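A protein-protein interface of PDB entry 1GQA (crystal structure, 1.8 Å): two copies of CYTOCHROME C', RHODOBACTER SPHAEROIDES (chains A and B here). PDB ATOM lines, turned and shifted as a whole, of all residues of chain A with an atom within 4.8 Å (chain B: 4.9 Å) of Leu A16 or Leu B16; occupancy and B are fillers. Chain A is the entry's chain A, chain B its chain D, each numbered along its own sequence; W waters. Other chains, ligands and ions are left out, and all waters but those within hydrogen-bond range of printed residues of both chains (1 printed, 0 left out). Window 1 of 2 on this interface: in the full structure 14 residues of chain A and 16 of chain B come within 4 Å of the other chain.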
ATOM      1  N   ALA A   9      -7.604  -5.286  24.467  1.00  0.00           N
ATOM      2  CA  ALA A   9      -8.994  -5.562  24.132  1.00  0.00           C
ATOM      3  C   ALA A   9      -9.951  -4.528  24.702  1.00  0.00           C
ATOM      4  O   ALA A   9     -10.927  -4.186  24.082  1.00  0.00           O
ATOM      5  CB  ALA A   9      -9.419  -7.003  24.530  1.00  0.00           C
ATOM      6  N   GLY A  12      -9.701  -1.446  22.739  1.00  0.00           N
ATOM      7  CA  GLY A  12     -10.288  -1.712  21.429  1.00  0.00           C
ATOM      8  C   GLY A  12     -11.806  -1.575  21.520  1.00  0.00           C
ATOM      9  O   GLY A  12     -12.433  -1.022  20.604  1.00  0.00           O
ATOM     10  N   TYR A  13     -12.395  -2.123  22.592  1.00  0.00           N
ATOM     11  CA  TYR A  13     -13.827  -2.090  22.840  1.00  0.00           C
ATOM     12  C   TYR A  13     -14.281  -0.628  22.821  1.00  0.00           C
ATOM     13  O   TYR A  13     -15.230  -0.287  22.108  1.00  0.00           O
ATOM     14  CB  TYR A  13     -14.203  -2.758  24.172  1.00  0.00           C
ATOM     15  CG  TYR A  13     -15.683  -2.660  24.517  1.00  0.00           C
ATOM     16  CD1 TYR A  13     -16.613  -3.492  23.920  1.00  0.00           C
ATOM     17  CD2 TYR A  13     -16.136  -1.675  25.400  1.00  0.00           C
ATOM     18  CE1 TYR A  13     -17.954  -3.394  24.244  1.00  0.00           C
ATOM     19  CE2 TYR A  13     -17.458  -1.541  25.711  1.00  0.00           C
ATOM     20  CZ  TYR A  13     -18.371  -2.406  25.111  1.00  0.00           C
ATOM     21  OH  TYR A  13     -19.705  -2.283  25.408  1.00  0.00           O
ATOM     22  N   PHE A  14     -13.617   0.232  23.576  1.00  0.00           N
ATOM     23  CA  PHE A  14     -14.043   1.625  23.576  1.00  0.00           C
ATOM     24  C   PHE A  14     -13.734   2.297  22.251  1.00  0.00           C
ATOM     25  O   PHE A  14     -14.455   3.184  21.875  1.00  0.00           O
ATOM     26  CB  PHE A  14     -13.533   2.437  24.807  1.00  0.00           C
ATOM     27  CG  PHE A  14     -14.154   1.976  26.077  1.00  0.00           C
ATOM     28  CD1 PHE A  14     -15.460   2.293  26.330  1.00  0.00           C
ATOM     29  CD2 PHE A  14     -13.485   1.152  26.970  1.00  0.00           C
ATOM     30  CE1 PHE A  14     -16.159   1.804  27.460  1.00  0.00           C
ATOM     31  CE2 PHE A  14     -14.152   0.657  28.118  1.00  0.00           C
ATOM     32  CZ  PHE A  14     -15.448   0.998  28.394  1.00  0.00           C
ATOM     33  N   SER A  15     -12.675   1.865  21.545  1.00  0.00           N
ATOM     34  CA  SER A  15     -12.409   2.427  20.213  1.00  0.00           C
ATOM     35  C   SER A  15     -13.622   2.200  19.288  1.00  0.00           C
ATOM     36  O   SER A  15     -13.989   3.100  18.510  1.00  0.00           O
ATOM     37  CB  SER A  15     -11.171   1.824  19.581  1.00  0.00           C
ATOM     38  OG  SER A  15     -10.031   2.364  20.169  1.00  0.00           O
ATOM     39  N   LEU A  16     -14.248   1.020  19.399  1.00  0.00           N
ATOM     40  CA  LEU A  16     -15.394   0.709  18.558  1.00  0.00           C
ATOM     41  C   LEU A  16     -16.595   1.580  18.947  1.00  0.00           C
ATOM     42  O   LEU A  16     -17.301   2.094  18.087  1.00  0.00           O
ATOM     43  CB  LEU A  16     -15.774  -0.774  18.639  1.00  0.00           C
ATOM     44  CG  LEU A  16     -14.769  -1.800  18.078  1.00  0.00           C
ATOM     45  CD1 LEU A  16     -15.078  -3.163  18.654  1.00  0.00           C
ATOM     46  CD2 LEU A  16     -14.990  -1.825  16.532  1.00  0.00           C
ATOM     47  N   VAL A  17     -16.858   1.665  20.249  1.00  0.00           N
ATOM     48  CA  VAL A  17     -17.907   2.496  20.769  1.00  0.00           C
ATOM     49  C   VAL A  17     -17.682   3.918  20.210  1.00  0.00           C
ATOM     50  O   VAL A  17     -18.570   4.504  19.649  1.00  0.00           O
ATOM     51  CB  VAL A  17     -17.845   2.534  22.273  1.00  0.00           C
ATOM     52  CG1 VAL A  17     -18.772   3.570  22.828  1.00  0.00           C
ATOM     53  CG2 VAL A  17     -18.132   1.184  22.816  1.00  0.00           C
ATOM     54  N   ALA A  18     -16.470   4.449  20.334  1.00  0.00           N
ATOM     55  CA  ALA A  18     -16.229   5.804  19.878  1.00  0.00           C
ATOM     56  C   ALA A  18     -16.449   5.910  18.347  1.00  0.00           C
ATOM     57  O   ALA A  18     -16.982   6.912  17.867  1.00  0.00           O
ATOM     58  CB  ALA A  18     -14.849   6.243  20.244  1.00  0.00           C
ATOM     59  N   LEU A  19     -16.038   4.881  17.615  1.00  0.00           N
ATOM     60  CA  LEU A  19     -16.183   4.875  16.155  1.00  0.00           C
ATOM     61  C   LEU A  19     -17.627   4.993  15.726  1.00  0.00           C
ATOM     62  O   LEU A  19     -17.928   5.709  14.789  1.00  0.00           O
ATOM     63  CB  LEU A  19     -15.582   3.605  15.567  1.00  0.00           C
ATOM     64  CG  LEU A  19     -15.141   3.613  14.085  1.00  0.00           C
ATOM     65  CD1 LEU A  19     -16.317   3.676  13.245  1.00  0.00           C
ATOM     66  CD2 LEU A  19     -14.275   4.727  13.722  1.00  0.00           C
ATOM     67  N   GLU A  20     -18.517   4.254  16.391  1.00  0.00           N
ATOM     68  CA  GLU A  20     -19.929   4.269  16.027  1.00  0.00           C
ATOM     69  C   GLU A  20     -20.693   5.485  16.565  1.00  0.00           C
ATOM     70  O   GLU A  20     -21.641   5.964  15.920  1.00  0.00           O
ATOM     71  CB  GLU A  20     -20.614   2.987  16.495  1.00  0.00           C
ATOM     72  CG  GLU A  20     -20.070   1.725  15.840  1.00  0.00           C
ATOM     73  CD  GLU A  20     -20.302   1.729  14.341  1.00  0.00           C
ATOM     74  OE1 GLU A  20     -21.283   2.349  13.853  1.00  0.00           O
ATOM     75  OE2 GLU A  20     -19.508   1.093  13.631  1.00  0.00           O
ATOM     76  N   LEU A  49     -22.862  -3.682  20.294  1.00  0.00           N
ATOM     77  CA  LEU A  49     -21.787  -3.491  21.227  1.00  0.00           C
ATOM     78  C   LEU A  49     -22.206  -3.544  22.683  1.00  0.00           C
ATOM     79  O   LEU A  49     -21.448  -4.052  23.494  1.00  0.00           O
ATOM     80  CB  LEU A  49     -21.081  -2.185  20.970  1.00  0.00           C
ATOM     81  CG  LEU A  49     -20.401  -2.136  19.623  1.00  0.00           C
ATOM     82  CD1 LEU A  49     -19.530  -0.875  19.558  1.00  0.00           C
ATOM     83  CD2 LEU A  49     -19.629  -3.467  19.337  1.00  0.00           C
ATOM     84  N   TYR A  52     -22.685  -7.176  23.946  1.00  0.00           N
ATOM     85  CA  TYR A  52     -21.462  -7.898  24.252  1.00  0.00           C
ATOM     86  C   TYR A  52     -21.180  -7.836  25.742  1.00  0.00           C
ATOM     87  O   TYR A  52     -21.166  -6.771  26.345  1.00  0.00           O
ATOM     88  CB  TYR A  52     -20.305  -7.258  23.485  1.00  0.00           C
ATOM     89  CG  TYR A  52     -18.957  -7.843  23.786  1.00  0.00           C
ATOM     90  CD1 TYR A  52     -18.543  -9.027  23.196  1.00  0.00           C
ATOM     91  CD2 TYR A  52     -18.083  -7.191  24.613  1.00  0.00           C
ATOM     92  CE1 TYR A  52     -17.300  -9.567  23.478  1.00  0.00           C
ATOM     93  CE2 TYR A  52     -16.846  -7.703  24.901  1.00  0.00           C
ATOM     94  CZ  TYR A  52     -16.452  -8.895  24.331  1.00  0.00           C
ATOM     95  OH  TYR A  52     -15.194  -9.393  24.631  1.00  0.00           O
ATOM     96  N   LEU A  57     -13.106  -8.286  29.888  1.00  0.00           N
ATOM     97  CA  LEU A  57     -12.308  -7.067  29.734  1.00  0.00           C
ATOM     98  C   LEU A  57     -11.818  -6.539  31.072  1.00  0.00           C
ATOM     99  O   LEU A  57     -10.928  -5.736  31.137  1.00  0.00           O
ATOM    100  CB  LEU A  57     -13.109  -5.949  29.045  1.00  0.00           C
ATOM    101  CG  LEU A  57     -13.613  -6.234  27.630  1.00  0.00           C
ATOM    102  CD1 LEU A  57     -14.498  -5.053  27.099  1.00  0.00           C
ATOM    103  CD2 LEU A  57     -12.482  -6.442  26.725  1.00  0.00           C
ATOM    104  N   ALA B   9      -9.833   0.988  15.687  1.00  0.00           N
ATOM    105  CA  ALA B   9     -11.047   0.191  15.909  1.00  0.00           C
ATOM    106  C   ALA B   9     -10.939  -1.180  15.229  1.00  0.00           C
ATOM    107  O   ALA B   9     -11.360  -2.153  15.808  1.00  0.00           O
ATOM    108  CB  ALA B   9     -12.315   0.914  15.492  1.00  0.00           C
ATOM    109  N   GLY B  12      -8.740  -3.161  17.312  1.00  0.00           N
ATOM    110  CA  GLY B  12      -9.553  -3.403  18.501  1.00  0.00           C
ATOM    111  C   GLY B  12     -10.554  -4.545  18.342  1.00  0.00           C
ATOM    112  O   GLY B  12     -10.682  -5.367  19.245  1.00  0.00           O
ATOM    113  N   TYR B  13     -11.291  -4.564  17.232  1.00  0.00           N
ATOM    114  CA  TYR B  13     -12.223  -5.637  16.854  1.00  0.00           C
ATOM    115  C   TYR B  13     -11.505  -7.020  16.858  1.00  0.00           C
ATOM    116  O   TYR B  13     -11.989  -7.965  17.482  1.00  0.00           O
ATOM    117  CB  TYR B  13     -12.817  -5.371  15.452  1.00  0.00           C
ATOM    118  CG  TYR B  13     -13.730  -6.460  15.001  1.00  0.00           C
ATOM    119  CD1 TYR B  13     -15.020  -6.546  15.491  1.00  0.00           C
ATOM    120  CD2 TYR B  13     -13.280  -7.454  14.160  1.00  0.00           C
ATOM    121  CE1 TYR B  13     -15.874  -7.548  15.086  1.00  0.00           C
ATOM    122  CE2 TYR B  13     -14.121  -8.497  13.777  1.00  0.00           C
ATOM    123  CZ  TYR B  13     -15.427  -8.523  14.253  1.00  0.00           C
ATOM    124  OH  TYR B  13     -16.288  -9.539  13.936  1.00  0.00           O
ATOM    125  N   PHE B  14     -10.325  -7.110  16.263  1.00  0.00           N
ATOM    126  CA  PHE B  14      -9.587  -8.396  16.280  1.00  0.00           C
ATOM    127  C   PHE B  14      -9.015  -8.725  17.672  1.00  0.00           C
ATOM    128  O   PHE B  14      -8.889  -9.899  18.035  1.00  0.00           O
ATOM    129  CB  PHE B  14      -8.559  -8.529  15.107  1.00  0.00           C
ATOM    130  CG  PHE B  14      -9.244  -8.681  13.797  1.00  0.00           C
ATOM    131  CD1 PHE B  14      -9.948  -9.836  13.510  1.00  0.00           C
ATOM    132  CD2 PHE B  14      -9.302  -7.636  12.901  1.00  0.00           C
ATOM    133  CE1 PHE B  14     -10.667  -9.963  12.277  1.00  0.00           C
ATOM    134  CE2 PHE B  14     -10.039  -7.754  11.705  1.00  0.00           C
ATOM    135  CZ  PHE B  14     -10.707  -8.909  11.396  1.00  0.00           C
ATOM    136  N   SER B  15      -8.713  -7.702  18.462  1.00  0.00           N
ATOM    137  CA  SER B  15      -8.247  -7.955  19.846  1.00  0.00           C
ATOM    138  C   SER B  15      -9.330  -8.587  20.692  1.00  0.00           C
ATOM    139  O   SER B  15      -9.020  -9.394  21.595  1.00  0.00           O
ATOM    140  CB  SER B  15      -7.825  -6.656  20.529  1.00  0.00           C
ATOM    141  OG  SER B  15      -6.679  -6.175  19.891  1.00  0.00           O
ATOM    142  N   LEU B  16     -10.590  -8.217  20.425  1.00  0.00           N
ATOM    143  CA  LEU B  16     -11.734  -8.790  21.140  1.00  0.00           C
ATOM    144  C   LEU B  16     -11.958 -10.210  20.623  1.00  0.00           C
ATOM    145  O   LEU B  16     -12.103 -11.089  21.434  1.00  0.00           O
ATOM    146  CB  LEU B  16     -12.986  -7.950  20.978  1.00  0.00           C
ATOM    147  CG  LEU B  16     -13.002  -6.575  21.616  1.00  0.00           C
ATOM    148  CD1 LEU B  16     -14.171  -5.761  20.965  1.00  0.00           C
ATOM    149  CD2 LEU B  16     -13.261  -6.685  23.130  1.00  0.00           C
ATOM    150  N   VAL B  17     -12.005 -10.406  19.288  1.00  0.00           N
ATOM    151  CA  VAL B  17     -12.093 -11.751  18.706  1.00  0.00           C
ATOM    152  C   VAL B  17     -11.014 -12.661  19.324  1.00  0.00           C
ATOM    153  O   VAL B  17     -11.312 -13.759  19.834  1.00  0.00           O
ATOM    154  CB  VAL B  17     -12.003 -11.742  17.151  1.00  0.00           C
ATOM    155  CG1 VAL B  17     -11.929 -13.145  16.530  1.00  0.00           C
ATOM    156  CG2 VAL B  17     -13.170 -10.979  16.520  1.00  0.00           C
ATOM    157  N   ALA B  18      -9.776 -12.207  19.354  1.00  0.00           N
ATOM    158  CA  ALA B  18      -8.709 -13.003  19.948  1.00  0.00           C
ATOM    159  C   ALA B  18      -8.926 -13.276  21.444  1.00  0.00           C
ATOM    160  O   ALA B  18      -8.670 -14.409  21.909  1.00  0.00           O
ATOM    161  CB  ALA B  18      -7.372 -12.350  19.785  1.00  0.00           C
ATOM    162  N   LEU B  19      -9.376 -12.261  22.199  1.00  0.00           N
ATOM    163  CA  LEU B  19      -9.579 -12.439  23.651  1.00  0.00           C
ATOM    164  C   LEU B  19     -10.538 -13.562  23.960  1.00  0.00           C
ATOM    165  O   LEU B  19     -10.313 -14.376  24.884  1.00  0.00           O
ATOM    166  CB  LEU B  19     -10.000 -11.134  24.324  1.00  0.00           C
ATOM    167  CG  LEU B  19     -10.111 -11.255  25.849  1.00  0.00           C
ATOM    168  CD1 LEU B  19      -8.720 -11.281  26.413  1.00  0.00           C
ATOM    169  CD2 LEU B  19     -10.869 -10.103  26.424  1.00  0.00           C
ATOM    170  N   GLU B  20     -11.590 -13.671  23.152  1.00  0.00           N
ATOM    171  CA  GLU B  20     -12.637 -14.681  23.389  1.00  0.00           C
ATOM    172  C   GLU B  20     -12.266 -16.038  22.817  1.00  0.00           C
ATOM    173  O   GLU B  20     -12.529 -17.075  23.420  1.00  0.00           O
ATOM    174  CB  GLU B  20     -13.975 -14.218  22.826  1.00  0.00           C
ATOM    175  CG  GLU B  20     -14.527 -12.994  23.523  1.00  0.00           C
ATOM    176  CD  GLU B  20     -14.750 -13.202  24.996  1.00  0.00           C
ATOM    177  OE1 GLU B  20     -15.035 -14.354  25.373  1.00  0.00           O
ATOM    178  OE2 GLU B  20     -14.647 -12.198  25.774  1.00  0.00           O
ATOM    179  N   LEU B  49     -19.883 -10.977  18.460  1.00  0.00           N
ATOM    180  CA  LEU B  49     -18.920 -10.209  17.656  1.00  0.00           C
ATOM    181  C   LEU B  49     -19.149 -10.401  16.156  1.00  0.00           C
ATOM    182  O   LEU B  49     -19.060  -9.445  15.403  1.00  0.00           O
ATOM    183  CB  LEU B  49     -17.489 -10.510  18.010  1.00  0.00           C
ATOM    184  CG  LEU B  49     -17.034 -10.120  19.398  1.00  0.00           C
ATOM    185  CD1 LEU B  49     -15.649 -10.708  19.658  1.00  0.00           C
ATOM    186  CD2 LEU B  49     -17.060  -8.610  19.546  1.00  0.00           C
ATOM    187  N   TYR B  52     -21.791  -8.014  14.778  1.00  0.00           N
ATOM    188  CA  TYR B  52     -21.438  -6.619  14.627  1.00  0.00           C
ATOM    189  C   TYR B  52     -21.118  -6.435  13.155  1.00  0.00           C
ATOM    190  O   TYR B  52     -20.315  -7.149  12.613  1.00  0.00           O
ATOM    191  CB  TYR B  52     -20.217  -6.316  15.490  1.00  0.00           C
ATOM    192  CG  TYR B  52     -19.667  -4.937  15.315  1.00  0.00           C
ATOM    193  CD1 TYR B  52     -20.268  -3.842  15.949  1.00  0.00           C
ATOM    194  CD2 TYR B  52     -18.548  -4.721  14.527  1.00  0.00           C
ATOM    195  CE1 TYR B  52     -19.782  -2.569  15.774  1.00  0.00           C
ATOM    196  CE2 TYR B  52     -18.071  -3.455  14.315  1.00  0.00           C
ATOM    197  CZ  TYR B  52     -18.685  -2.386  14.949  1.00  0.00           C
ATOM    198  OH  TYR B  52     -18.211  -1.130  14.763  1.00  0.00           O
ATOM    199  N   LEU B  57     -15.222  -0.520   9.643  1.00  0.00           N
ATOM    200  CA  LEU B  57     -13.828  -0.844   9.899  1.00  0.00           C
ATOM    201  C   LEU B  57     -13.011  -0.867   8.602  1.00  0.00           C
ATOM    202  O   LEU B  57     -11.803  -0.751   8.617  1.00  0.00           O
ATOM    203  CB  LEU B  57     -13.721  -2.214  10.583  1.00  0.00           C
ATOM    204  CG  LEU B  57     -14.396  -2.325  11.941  1.00  0.00           C
ATOM    205  CD1 LEU B  57     -14.197  -3.757  12.537  1.00  0.00           C
ATOM    206  CD2 LEU B  57     -13.930  -1.234  12.866  1.00  0.00           C
HETATM  207  O   HOH W   1     -18.642  -1.331  11.455  1.00  0.00           O
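Water W1 bridges OH of Tyr B52 and OE2 of Glu A20.
Among the printed residues, 14 pairs touch across the chains.
Among the printed residues, no Asp or Glu carboxylate lies within 4 Å of a Lys or Arg side-chain nitrogen of the other chain.
Of chain A, only Ala A9 (3.5 Å), Leu A16 (3.6 Å), Tyr A52 (3.7 Å) and Leu A57 (3.7 Å) come within 4 Å of Leu B16.
Printed residues of chain A within 4 Å of Gly B12: Gly A12 (3.5 Å).
Of the printed residues of chain B, Gly A12 touches Gly B12.
Printed residues of chain A within 4 Å of Leu B49: Tyr A52.
The nearest residue of chain A that does not touch Leu B16 is Tyr A13 (4.1 Å).
CB of Ala A9 touches O of Ser B15, 3.8 Å away.
CD2 of Leu B16 touches O of Ala A9, at 3.5 Å.
Ala A9 touches Leu B19.
Gly B12 touches Gly A12.
Leu B16 touches Leu A16.
Tyr B52 touches Leu A16.
Leu A16 touches Leu B57.
CD1 of Tyr B52 touches CD2 of Leu A49 (3.5 Å).
Tyr A52 touches Leu B16.
CD2 of Leu B49 touches CD1 of Tyr A52 (3.96 Å).
Ala A9 touches Leu B19, but with the chains exchanged Leu A19 does not touch Ala B9 (4.2 Å).
Leu A16 touches its own counterpart, Leu B16.
Leu A16 touches Tyr B52, and with the chains exchanged Tyr A52 touches Leu B16.
Leu A16 touches Leu B57, and with the chains exchanged Leu A57 touches Leu B16.
13 positions are printed for both chains.
Of the 14 pairs that touch across the chains among the printed residues, 12 have their exchanged pair printed and touching as well.
OE2 of Glu B20 sits at hydrogen-bond distance from OH of Tyr A52 (3.1 Å).
OE2 of Glu A20 lies within hydrogen-bond range of OH of Tyr B52.
O of Leu A49 is in hydrogen-bond range of OH of Tyr A13 (3.1 Å).
The side-chain hydroxyl (OH) of Tyr B13 sits at hydrogen-bond distance from the backbone carbonyl oxygen (O) of Leu B49 (3.1 Å).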
